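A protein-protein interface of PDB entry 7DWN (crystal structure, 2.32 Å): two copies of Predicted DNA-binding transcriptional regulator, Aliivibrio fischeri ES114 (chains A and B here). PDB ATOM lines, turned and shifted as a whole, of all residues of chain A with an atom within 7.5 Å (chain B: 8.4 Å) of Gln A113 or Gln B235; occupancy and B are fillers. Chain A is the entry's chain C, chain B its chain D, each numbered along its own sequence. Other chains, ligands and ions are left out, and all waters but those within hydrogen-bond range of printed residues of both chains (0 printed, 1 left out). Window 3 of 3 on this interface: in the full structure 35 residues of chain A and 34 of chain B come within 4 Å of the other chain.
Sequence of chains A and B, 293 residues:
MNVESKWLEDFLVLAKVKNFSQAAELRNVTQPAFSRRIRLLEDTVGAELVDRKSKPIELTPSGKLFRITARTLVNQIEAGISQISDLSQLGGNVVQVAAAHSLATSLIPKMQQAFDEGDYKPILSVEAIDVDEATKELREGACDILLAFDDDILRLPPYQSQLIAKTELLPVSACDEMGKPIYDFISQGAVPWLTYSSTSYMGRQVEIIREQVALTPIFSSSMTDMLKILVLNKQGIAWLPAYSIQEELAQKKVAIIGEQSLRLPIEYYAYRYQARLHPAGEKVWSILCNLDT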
ATOM      1  N   LEU A 107      14.311  -0.654  -7.564  1.00  0.00           N
ATOM      2  CA  LEU A 107      14.262  -1.866  -6.755  1.00  0.00           C
ATOM      3  C   LEU A 107      14.189  -1.597  -5.258  1.00  0.00           C
ATOM      4  O   LEU A 107      13.455  -2.296  -4.549  1.00  0.00           O
ATOM      5  CB  LEU A 107      15.482  -2.743  -7.053  1.00  0.00           C
ATOM      6  CG  LEU A 107      15.610  -3.313  -8.466  1.00  0.00           C
ATOM      7  CD1 LEU A 107      16.721  -4.356  -8.521  1.00  0.00           C
ATOM      8  CD2 LEU A 107      14.289  -3.899  -8.943  1.00  0.00           C
ATOM      9  N   ILE A 108      14.944  -0.618  -4.744  1.00  0.00           N
ATOM     10  CA  ILE A 108      15.003  -0.419  -3.293  1.00  0.00           C
ATOM     11  C   ILE A 108      13.641  -0.116  -2.680  1.00  0.00           C
ATOM     12  O   ILE A 108      13.339  -0.664  -1.608  1.00  0.00           O
ATOM     13  CB  ILE A 108      16.056   0.656  -2.949  1.00  0.00           C
ATOM     14  CG1 ILE A 108      17.436   0.020  -2.760  1.00  0.00           C
ATOM     15  CG2 ILE A 108      15.663   1.405  -1.682  1.00  0.00           C
ATOM     16  CD1 ILE A 108      18.086  -0.462  -4.033  1.00  0.00           C
ATOM     17  N   PRO A 109      12.784   0.733  -3.273  1.00  0.00           N
ATOM     18  CA  PRO A 109      11.506   1.038  -2.604  1.00  0.00           C
ATOM     19  C   PRO A 109      10.637  -0.178  -2.323  1.00  0.00           C
ATOM     20  O   PRO A 109      10.027  -0.251  -1.248  1.00  0.00           O
ATOM     21  CB  PRO A 109      10.826   2.018  -3.574  1.00  0.00           C
ATOM     22  CG  PRO A 109      11.589   1.907  -4.856  1.00  0.00           C
ATOM     23  CD  PRO A 109      12.981   1.592  -4.452  1.00  0.00           C
ATOM     24  N   LYS A 110      10.556  -1.141  -3.246  1.00  0.00           N
ATOM     25  CA  LYS A 110       9.722  -2.312  -2.990  1.00  0.00           C
ATOM     26  C   LYS A 110      10.379  -3.249  -1.981  1.00  0.00           C
ATOM     27  O   LYS A 110       9.689  -3.882  -1.174  1.00  0.00           O
ATOM     28  CB  LYS A 110       9.411  -3.043  -4.299  1.00  0.00           C
ATOM     29  CG  LYS A 110      10.624  -3.539  -5.063  1.00  0.00           C
ATOM     30  CD  LYS A 110      10.227  -4.106  -6.419  1.00  0.00           C
ATOM     31  CE  LYS A 110       9.573  -3.045  -7.292  1.00  0.00           C
ATOM     32  NZ  LYS A 110       9.235  -3.565  -8.646  1.00  0.00           N
ATOM     33  N   MET A 111      11.711  -3.347  -2.010  1.00  0.00           N
ATOM     34  CA  MET A 111      12.425  -4.103  -0.985  1.00  0.00           C
ATOM     35  C   MET A 111      12.172  -3.527   0.399  1.00  0.00           C
ATOM     36  O   MET A 111      12.036  -4.272   1.377  1.00  0.00           O
ATOM     37  CB  MET A 111      13.924  -4.098  -1.274  1.00  0.00           C
ATOM     38  CG  MET A 111      14.403  -5.163  -2.227  1.00  0.00           C
ATOM     39  SD  MET A 111      16.200  -5.134  -2.318  1.00  0.00           S
ATOM     40  CE  MET A 111      16.470  -3.724  -3.387  1.00  0.00           C
ATOM     41  N   GLN A 112      12.113  -2.197   0.498  1.00  0.00           N
ATOM     42  CA  GLN A 112      12.013  -1.535   1.792  1.00  0.00           C
ATOM     43  C   GLN A 112      10.724  -1.891   2.517  1.00  0.00           C
ATOM     44  O   GLN A 112      10.695  -1.921   3.752  1.00  0.00           O
ATOM     45  CB  GLN A 112      12.118  -0.021   1.607  1.00  0.00           C
ATOM     46  CG  GLN A 112      13.466   0.557   1.994  1.00  0.00           C
ATOM     47  CD  GLN A 112      13.705   0.499   3.486  1.00  0.00           C
ATOM     48  OE1 GLN A 112      12.800   0.754   4.281  1.00  0.00           O
ATOM     49  NE2 GLN A 112      14.925   0.153   3.878  1.00  0.00           N
ATOM     50  N   GLN A 113       9.656  -2.167   1.775  1.00  0.00           N
ATOM     51  CA  GLN A 113       8.367  -2.466   2.379  1.00  0.00           C
ATOM     52  C   GLN A 113       8.194  -3.941   2.719  1.00  0.00           C
ATOM     53  O   GLN A 113       7.278  -4.283   3.473  1.00  0.00           O
ATOM     54  CB  GLN A 113       7.237  -2.006   1.450  1.00  0.00           C
ATOM     55  CG  GLN A 113       5.909  -1.801   2.157  1.00  0.00           C
ATOM     56  CD  GLN A 113       6.061  -1.050   3.466  1.00  0.00           C
ATOM     57  OE1 GLN A 113       6.693   0.006   3.522  1.00  0.00           O
ATOM     58  NE2 GLN A 113       5.488  -1.599   4.531  1.00  0.00           N
ATOM     59  N   ALA A 114       9.050  -4.815   2.198  1.00  0.00           N
ATOM     60  CA  ALA A 114       8.967  -6.243   2.475  1.00  0.00           C
ATOM     61  C   ALA A 114       9.699  -6.650   3.748  1.00  0.00           C
ATOM     62  O   ALA A 114       9.642  -7.824   4.128  1.00  0.00           O
ATOM     63  CB  ALA A 114       9.515  -7.043   1.289  1.00  0.00           C
ATOM     64  N   PHE A 115      10.379  -5.719   4.413  1.00  0.00           N
ATOM     65  CA  PHE A 115      11.134  -6.044   5.616  1.00  0.00           C
ATOM     66  C   PHE A 115      10.204  -6.236   6.809  1.00  0.00           C
ATOM     67  O   PHE A 115       9.245  -5.483   6.995  1.00  0.00           O
ATOM     68  CB  PHE A 115      12.146  -4.938   5.924  1.00  0.00           C
ATOM     69  CG  PHE A 115      13.249  -4.817   4.910  1.00  0.00           C
ATOM     70  CD1 PHE A 115      13.693  -5.924   4.209  1.00  0.00           C
ATOM     71  CD2 PHE A 115      13.850  -3.593   4.665  1.00  0.00           C
ATOM     72  CE1 PHE A 115      14.713  -5.811   3.280  1.00  0.00           C
ATOM     73  CE2 PHE A 115      14.867  -3.476   3.736  1.00  0.00           C
ATOM     74  CZ  PHE A 115      15.298  -4.588   3.043  1.00  0.00           C
ATOM     75  N   ASP A 116      10.498  -7.248   7.619  1.00  0.00           N
ATOM     76  CA  ASP A 116       9.781  -7.486   8.862  1.00  0.00           C
ATOM     77  C   ASP A 116      10.442  -6.717  10.006  1.00  0.00           C
ATOM     78  O   ASP A 116      11.602  -6.315   9.919  1.00  0.00           O
ATOM     79  CB  ASP A 116       9.727  -8.980   9.180  1.00  0.00           C
ATOM     80  CG  ASP A 116       9.008  -9.777   8.106  1.00  0.00           C
ATOM     81  OD1 ASP A 116       9.600  -9.990   7.026  1.00  0.00           O
ATOM     82  OD2 ASP A 116       7.850 -10.183   8.339  1.00  0.00           O
ATOM     83  N   GLU A 117       9.689  -6.532  11.091  1.00  0.00           N
ATOM     84  CA  GLU A 117      10.032  -5.564  12.126  1.00  0.00           C
ATOM     85  C   GLU A 117      10.994  -6.090  13.193  1.00  0.00           C
ATOM     86  O   GLU A 117      11.216  -5.404  14.189  1.00  0.00           O
ATOM     87  CB  GLU A 117       8.749  -5.067  12.812  1.00  0.00           C
ATOM     88  CG  GLU A 117       7.861  -4.219  11.918  1.00  0.00           C
ATOM     89  CD  GLU A 117       8.548  -2.952  11.458  1.00  0.00           C
ATOM     90  OE1 GLU A 117       9.309  -2.374  12.262  1.00  0.00           O
ATOM     91  OE2 GLU A 117       8.333  -2.542  10.296  1.00  0.00           O
ATOM     92  N   LYS A 121      16.055  -7.025  11.181  1.00  0.00           N
ATOM     93  CA  LYS A 121      15.514  -6.248  10.073  1.00  0.00           C
ATOM     94  C   LYS A 121      16.635  -5.471   9.400  1.00  0.00           C
ATOM     95  O   LYS A 121      17.289  -4.651  10.057  1.00  0.00           O
ATOM     96  CB  LYS A 121      14.433  -5.284  10.542  1.00  0.00           C
ATOM     97  CG  LYS A 121      13.992  -4.323   9.444  1.00  0.00           C
ATOM     98  CD  LYS A 121      12.869  -3.403   9.886  1.00  0.00           C
ATOM     99  CE  LYS A 121      12.429  -2.507   8.737  1.00  0.00           C
ATOM    100  NZ  LYS A 121      11.315  -1.596   9.119  1.00  0.00           N
ATOM    101  N   SER B 173       8.358  15.833   4.787  1.00  0.00           N
ATOM    102  CA  SER B 173       7.609  14.609   5.011  1.00  0.00           C
ATOM    103  C   SER B 173       6.472  14.537   4.002  1.00  0.00           C
ATOM    104  O   SER B 173       5.918  15.562   3.591  1.00  0.00           O
ATOM    105  CB  SER B 173       7.037  14.549   6.436  1.00  0.00           C
ATOM    106  OG  SER B 173       6.046  13.542   6.558  1.00  0.00           O
ATOM    107  N   ALA B 174       6.133  13.318   3.600  1.00  0.00           N
ATOM    108  CA  ALA B 174       4.939  13.118   2.797  1.00  0.00           C
ATOM    109  C   ALA B 174       3.700  13.357   3.649  1.00  0.00           C
ATOM    110  O   ALA B 174       3.691  13.103   4.855  1.00  0.00           O
ATOM    111  CB  ALA B 174       4.909  11.707   2.214  1.00  0.00           C
ATOM    112  N   ILE B 182       2.496  13.291   7.356  1.00  0.00           N
ATOM    113  CA  ILE B 182       2.443  12.021   8.076  1.00  0.00           C
ATOM    114  C   ILE B 182       3.425  12.030   9.238  1.00  0.00           C
ATOM    115  O   ILE B 182       3.144  11.488  10.315  1.00  0.00           O
ATOM    116  CB  ILE B 182       2.708  10.854   7.106  1.00  0.00           C
ATOM    117  CG1 ILE B 182       1.644  10.838   6.007  1.00  0.00           C
ATOM    118  CG2 ILE B 182       2.733   9.528   7.849  1.00  0.00           C
ATOM    119  CD1 ILE B 182       1.904   9.829   4.922  1.00  0.00           C
ATOM    120  N   TYR B 183       4.582  12.657   9.049  1.00  0.00           N
ATOM    121  CA  TYR B 183       5.569  12.810  10.103  1.00  0.00           C
ATOM    122  C   TYR B 183       5.820  14.289  10.362  1.00  0.00           C
ATOM    123  O   TYR B 183       5.725  15.122   9.456  1.00  0.00           O
ATOM    124  CB  TYR B 183       6.891  12.122   9.745  1.00  0.00           C
ATOM    125  CG  TYR B 183       6.749  10.692   9.276  1.00  0.00           C
ATOM    126  CD1 TYR B 183       6.538   9.662  10.182  1.00  0.00           C
ATOM    127  CD2 TYR B 183       6.845  10.371   7.927  1.00  0.00           C
ATOM    128  CE1 TYR B 183       6.413   8.352   9.758  1.00  0.00           C
ATOM    129  CE2 TYR B 183       6.722   9.065   7.494  1.00  0.00           C
ATOM    130  CZ  TYR B 183       6.507   8.060   8.414  1.00  0.00           C
ATOM    131  OH  TYR B 183       6.384   6.757   7.988  1.00  0.00           O
ATOM    132  N   VAL B 191      11.516  10.338  14.837  1.00  0.00           N
ATOM    133  CA  VAL B 191      10.847  10.052  13.574  1.00  0.00           C
ATOM    134  C   VAL B 191      11.779   9.221  12.699  1.00  0.00           C
ATOM    135  O   VAL B 191      13.011   9.307  12.841  1.00  0.00           O
ATOM    136  CB  VAL B 191      10.404  11.347  12.874  1.00  0.00           C
ATOM    137  CG1 VAL B 191       9.551  12.180  13.816  1.00  0.00           C
ATOM    138  CG2 VAL B 191      11.603  12.143  12.390  1.00  0.00           C
ATOM    139  N   PRO B 192      11.238   8.381  11.816  1.00  0.00           N
ATOM    140  CA  PRO B 192      12.092   7.651  10.872  1.00  0.00           C
ATOM    141  C   PRO B 192      12.810   8.619   9.947  1.00  0.00           C
ATOM    142  O   PRO B 192      12.199   9.510   9.352  1.00  0.00           O
ATOM    143  CB  PRO B 192      11.104   6.757  10.114  1.00  0.00           C
ATOM    144  CG  PRO B 192       9.773   7.411  10.299  1.00  0.00           C
ATOM    145  CD  PRO B 192       9.816   8.033  11.661  1.00  0.00           C
ATOM    146  N   TRP B 193      14.120   8.433   9.824  1.00  0.00           N
ATOM    147  CA  TRP B 193      14.997   9.403   9.189  1.00  0.00           C
ATOM    148  C   TRP B 193      15.716   8.731   8.028  1.00  0.00           C
ATOM    149  O   TRP B 193      16.401   7.718   8.216  1.00  0.00           O
ATOM    150  CB  TRP B 193      15.988   9.955  10.215  1.00  0.00           C
ATOM    151  CG  TRP B 193      17.008  10.904   9.683  1.00  0.00           C
ATOM    152  CD1 TRP B 193      16.891  11.721   8.597  1.00  0.00           C
ATOM    153  CD2 TRP B 193      18.315  11.131  10.219  1.00  0.00           C
ATOM    154  NE1 TRP B 193      18.048  12.445   8.426  1.00  0.00           N
ATOM    155  CE2 TRP B 193      18.936  12.100   9.409  1.00  0.00           C
ATOM    156  CE3 TRP B 193      19.019  10.607  11.308  1.00  0.00           C
ATOM    157  CZ2 TRP B 193      20.229  12.555   9.652  1.00  0.00           C
ATOM    158  CZ3 TRP B 193      20.300  11.060  11.548  1.00  0.00           C
ATOM    159  CH2 TRP B 193      20.893  12.025  10.724  1.00  0.00           C
ATOM    160  N   LEU B 194      15.533   9.285   6.830  1.00  0.00           N
ATOM    161  CA  LEU B 194      16.241   8.862   5.626  1.00  0.00           C
ATOM    162  C   LEU B 194      17.381   9.849   5.409  1.00  0.00           C
ATOM    163  O   LEU B 194      17.144  11.013   5.070  1.00  0.00           O
ATOM    164  CB  LEU B 194      15.295   8.831   4.428  1.00  0.00           C
ATOM    165  CG  LEU B 194      13.929   8.185   4.676  1.00  0.00           C
ATOM    166  CD1 LEU B 194      12.945   8.573   3.587  1.00  0.00           C
ATOM    167  CD2 LEU B 194      14.054   6.676   4.769  1.00  0.00           C
ATOM    168  N   THR B 216      15.629   8.842  14.126  1.00  0.00           N
ATOM    169  CA  THR B 216      16.162   7.482  14.110  1.00  0.00           C
ATOM    170  C   THR B 216      16.506   7.107  12.678  1.00  0.00           C
ATOM    171  O   THR B 216      15.597   6.996  11.835  1.00  0.00           O
ATOM    172  CB  THR B 216      15.167   6.481  14.700  1.00  0.00           C
ATOM    173  OG1 THR B 216      13.837   6.823  14.290  1.00  0.00           O
ATOM    174  CG2 THR B 216      15.250   6.484  16.221  1.00  0.00           C
ATOM    175  N   ILE B 218      16.900   5.130   9.543  1.00  0.00           N
ATOM    176  CA  ILE B 218      16.433   3.835   9.059  1.00  0.00           C
ATOM    177  C   ILE B 218      16.910   3.533   7.653  1.00  0.00           C
ATOM    178  O   ILE B 218      16.580   2.464   7.117  1.00  0.00           O
ATOM    179  CB  ILE B 218      14.898   3.727   9.130  1.00  0.00           C
ATOM    180  CG1 ILE B 218      14.254   4.681   8.121  1.00  0.00           C
ATOM    181  CG2 ILE B 218      14.410   4.006  10.545  1.00  0.00           C
ATOM    182  CD1 ILE B 218      12.852   4.285   7.713  1.00  0.00           C
ATOM    183  N   PHE B 219      17.678   4.429   7.038  1.00  0.00           N
ATOM    184  CA  PHE B 219      18.065   4.284   5.643  1.00  0.00           C
ATOM    185  C   PHE B 219      19.093   5.351   5.307  1.00  0.00           C
ATOM    186  O   PHE B 219      18.975   6.490   5.765  1.00  0.00           O
ATOM    187  CB  PHE B 219      16.844   4.411   4.726  1.00  0.00           C
ATOM    188  CG  PHE B 219      17.158   4.261   3.273  1.00  0.00           C
ATOM    189  CD1 PHE B 219      17.155   3.011   2.680  1.00  0.00           C
ATOM    190  CD2 PHE B 219      17.448   5.371   2.498  1.00  0.00           C
ATOM    191  CE1 PHE B 219      17.439   2.869   1.341  1.00  0.00           C
ATOM    192  CE2 PHE B 219      17.731   5.235   1.160  1.00  0.00           C
ATOM    193  CZ  PHE B 219      17.724   3.982   0.582  1.00  0.00           C
ATOM    194  N   MET B 226      16.923   8.887  -4.290  1.00  0.00           N
ATOM    195  CA  MET B 226      16.507   7.756  -3.465  1.00  0.00           C
ATOM    196  C   MET B 226      15.765   8.225  -2.220  1.00  0.00           C
ATOM    197  O   MET B 226      14.687   7.710  -1.891  1.00  0.00           O
ATOM    198  CB  MET B 226      17.731   6.926  -3.079  1.00  0.00           C
ATOM    199  CG  MET B 226      17.400   5.669  -2.301  1.00  0.00           C
ATOM    200  SD  MET B 226      16.524   4.488  -3.332  1.00  0.00           S
ATOM    201  CE  MET B 226      17.455   4.703  -4.837  1.00  0.00           C
ATOM    202  N   LEU B 227      16.347   9.188  -1.500  1.00  0.00           N
ATOM    203  CA  LEU B 227      15.686   9.743  -0.326  1.00  0.00           C
ATOM    204  C   LEU B 227      14.337  10.344  -0.690  1.00  0.00           C
ATOM    205  O   LEU B 227      13.362  10.197   0.052  1.00  0.00           O
ATOM    206  CB  LEU B 227      16.578  10.798   0.329  1.00  0.00           C
ATOM    207  CG  LEU B 227      17.962  10.352   0.800  1.00  0.00           C
ATOM    208  CD1 LEU B 227      18.622  11.450   1.619  1.00  0.00           C
ATOM    209  CD2 LEU B 227      17.863   9.063   1.603  1.00  0.00           C
ATOM    210  N   LYS B 228      14.266  11.018  -1.839  1.00  0.00           N
ATOM    211  CA  LYS B 228      13.018  11.629  -2.282  1.00  0.00           C
ATOM    212  C   LYS B 228      11.954  10.571  -2.542  1.00  0.00           C
ATOM    213  O   LYS B 228      10.803  10.718  -2.119  1.00  0.00           O
ATOM    214  CB  LYS B 228      13.267  12.463  -3.539  1.00  0.00           C
ATOM    215  CG  LYS B 228      12.009  13.016  -4.185  1.00  0.00           C
ATOM    216  CD  LYS B 228      12.346  13.793  -5.449  1.00  0.00           C
ATOM    217  CE  LYS B 228      11.094  14.267  -6.167  1.00  0.00           C
ATOM    218  NZ  LYS B 228      11.420  14.949  -7.449  1.00  0.00           N
ATOM    219  N   ILE B 229      12.323   9.494  -3.241  1.00  0.00           N
ATOM    220  CA  ILE B 229      11.362   8.431  -3.521  1.00  0.00           C
ATOM    221  C   ILE B 229      10.880   7.792  -2.225  1.00  0.00           C
ATOM    222  O   ILE B 229       9.680   7.549  -2.046  1.00  0.00           O
ATOM    223  CB  ILE B 229      11.976   7.390  -4.474  1.00  0.00           C
ATOM    224  CG1 ILE B 229      12.158   7.993  -5.866  1.00  0.00           C
ATOM    225  CG2 ILE B 229      11.106   6.144  -4.539  1.00  0.00           C
ATOM    226  CD1 ILE B 229      12.809   7.064  -6.848  1.00  0.00           C
ATOM    227  N   LEU B 230      11.799   7.528  -1.292  1.00  0.00           N
ATOM    228  CA  LEU B 230      11.385   6.905  -0.039  1.00  0.00           C
ATOM    229  C   LEU B 230      10.536   7.845   0.810  1.00  0.00           C
ATOM    230  O   LEU B 230       9.668   7.383   1.559  1.00  0.00           O
ATOM    231  CB  LEU B 230      12.604   6.422   0.746  1.00  0.00           C
ATOM    232  CG  LEU B 230      13.301   5.184   0.180  1.00  0.00           C
ATOM    233  CD1 LEU B 230      14.295   4.641   1.180  1.00  0.00           C
ATOM    234  CD2 LEU B 230      12.287   4.116  -0.200  1.00  0.00           C
ATOM    235  N   VAL B 231      10.763   9.156   0.709  1.00  0.00           N
ATOM    236  CA  VAL B 231       9.875  10.116   1.360  1.00  0.00           C
ATOM    237  C   VAL B 231       8.489  10.055   0.733  1.00  0.00           C
ATOM    238  O   VAL B 231       7.471   9.984   1.432  1.00  0.00           O
ATOM    239  CB  VAL B 231      10.465  11.537   1.280  1.00  0.00           C
ATOM    240  CG1 VAL B 231       9.402  12.573   1.611  1.00  0.00           C
ATOM    241  CG2 VAL B 231      11.641  11.678   2.223  1.00  0.00           C
ATOM    242  N   LEU B 232       8.434  10.072  -0.601  1.00  0.00           N
ATOM    243  CA  LEU B 232       7.158  10.011  -1.306  1.00  0.00           C
ATOM    244  C   LEU B 232       6.416   8.714  -1.015  1.00  0.00           C
ATOM    245  O   LEU B 232       5.180   8.692  -1.021  1.00  0.00           O
ATOM    246  CB  LEU B 232       7.382  10.172  -2.811  1.00  0.00           C
ATOM    247  CG  LEU B 232       7.334  11.588  -3.399  1.00  0.00           C
ATOM    248  CD1 LEU B 232       8.334  12.515  -2.732  1.00  0.00           C
ATOM    249  CD2 LEU B 232       7.568  11.553  -4.903  1.00  0.00           C
ATOM    250  N   ASN B 233       7.144   7.627  -0.756  1.00  0.00           N
ATOM    251  CA  ASN B 233       6.538   6.359  -0.370  1.00  0.00           C
ATOM    252  C   ASN B 233       6.242   6.278   1.125  1.00  0.00           C
ATOM    253  O   ASN B 233       6.045   5.172   1.647  1.00  0.00           O
ATOM    254  CB  ASN B 233       7.433   5.193  -0.799  1.00  0.00           C
ATOM    255  CG  ASN B 233       7.505   5.037  -2.308  1.00  0.00           C
ATOM    256  OD1 ASN B 233       6.620   5.491  -3.034  1.00  0.00           O
ATOM    257  ND2 ASN B 233       8.562   4.390  -2.787  1.00  0.00           N
ATOM    258  N   LYS B 234       6.225   7.422   1.815  1.00  0.00           N
ATOM    259  CA  LYS B 234       5.782   7.521   3.207  1.00  0.00           C
ATOM    260  C   LYS B 234       6.667   6.716   4.156  1.00  0.00           C
ATOM    261  O   LYS B 234       6.207   6.246   5.199  1.00  0.00           O
ATOM    262  CB  LYS B 234       4.317   7.092   3.348  1.00  0.00           C
ATOM    263  CG  LYS B 234       3.394   7.692   2.294  1.00  0.00           C
ATOM    264  CD  LYS B 234       1.960   7.223   2.469  1.00  0.00           C
ATOM    265  CE  LYS B 234       1.095   7.664   1.298  1.00  0.00           C
ATOM    266  NZ  LYS B 234       1.281   9.107   0.981  1.00  0.00           N
ATOM    267  N   GLN B 235       7.947   6.559   3.814  1.00  0.00           N
ATOM    268  CA  GLN B 235       8.860   5.784   4.646  1.00  0.00           C
ATOM    269  C   GLN B 235       9.536   6.610   5.731  1.00  0.00           C
ATOM    270  O   GLN B 235      10.009   6.035   6.718  1.00  0.00           O
ATOM    271  CB  GLN B 235       9.933   5.114   3.781  1.00  0.00           C
ATOM    272  CG  GLN B 235       9.377   4.121   2.776  1.00  0.00           C
ATOM    273  CD  GLN B 235       8.518   3.056   3.430  1.00  0.00           C
ATOM    274  OE1 GLN B 235       8.994   2.280   4.260  1.00  0.00           O
ATOM    275  NE2 GLN B 235       7.241   3.021   3.066  1.00  0.00           N
ATOM    276  N   GLY B 236       9.595   7.928   5.580  1.00  0.00           N
ATOM    277  CA  GLY B 236      10.227   8.761   6.582  1.00  0.00           C
ATOM    278  C   GLY B 236      10.405  10.177   6.072  1.00  0.00           C
ATOM    279  O   GLY B 236       9.882  10.551   5.020  1.00  0.00           O
ATOM    280  N   ILE B 237      11.157  10.956   6.845  1.00  0.00           N
ATOM    281  CA  ILE B 237      11.433  12.346   6.520  1.00  0.00           C
ATOM    282  C   ILE B 237      12.849  12.446   5.974  1.00  0.00           C
ATOM    283  O   ILE B 237      13.706  11.596   6.235  1.00  0.00           O
ATOM    284  CB  ILE B 237      11.253  13.274   7.743  1.00  0.00           C
ATOM    285  CG1 ILE B 237      12.245  12.903   8.850  1.00  0.00           C
ATOM    286  CG2 ILE B 237       9.836  13.201   8.254  1.00  0.00           C
ATOM    287  CD1 ILE B 237      13.405  13.864   8.987  1.00  0.00           C
ATOM    288  N   ALA B 238      13.111  13.510   5.218  1.00  0.00           N
ATOM    289  CA  ALA B 238      14.475  13.703   4.742  1.00  0.00           C
ATOM    290  C   ALA B 238      14.726  15.176   4.453  1.00  0.00           C
ATOM    291  O   ALA B 238      13.800  15.937   4.170  1.00  0.00           O
ATOM    292  CB  ALA B 238      14.767  12.862   3.493  1.00  0.00           C
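The side-chain amide oxygen (OE1) of Gln A113 lies within hydrogen-bond range of the side-chain amide nitrogen (NE2) of Gln B235, at 3.1 Å.
The backbone carbonyl oxygen of Ile B229 lies close to the side-chain amide nitrogen of Asn B233 (3.4 Å).
O of Leu B230 is in hydrogen-bond range of N of Gln B235 (3.0 Å).
O of Asn B233 sits at hydrogen-bond distance from NE2 of Gln B235, 2.8 Å away.
No position is printed for both chains.
Of the 6 pairs that touch across the chains among the printed residues, none has its exchanged pair printed and touching as well.
Ile A108 touches Phe B219.
CG2 of Ile A108 touches SD of Met B226, at 3.6 Å.
Pro A109 touches Leu B230.
Pro A109 touches Asn B233.
NE2 of Gln A112 touches CD1 of Phe B219 (3.8 Å).
Gln A113 touches just one residue of chain B: Gln B235.
Of chain A, only Gln A113 (3.1 Å) comes within 4 Å of Gln B235.
Of the printed residues of chain B, Gln A112 touches Phe B219 (3.8 Å).
Of the printed residues of chain A, Phe B219 touches Ile A108 and Gln A112.
Of the printed residues of chain A, Met B226 touches Ile A108.
Of the printed residues of chain A, Asn B233 touches Pro A109.
Of the printed residues of chain B, Pro A109 touches Leu B230 and Asn B233.
Lys A110 touches none of the printed residues of chain B.
The nearest residue of chain B that does not touch Gln A113 is Asn B233 (5.5 Å).
Of the 12 printed residues of chain A, 4 touch a printed residue of chain B.
Along chain A the printed residues that touch a printed residue of chain B span positions 108 to 113.
Among the printed residues, 6 pairs touch across the chains.
Among the printed residues, no Asp or Glu carboxylate lies within 4 Å of a Lys or Arg side-chain nitrogen of the other chain.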
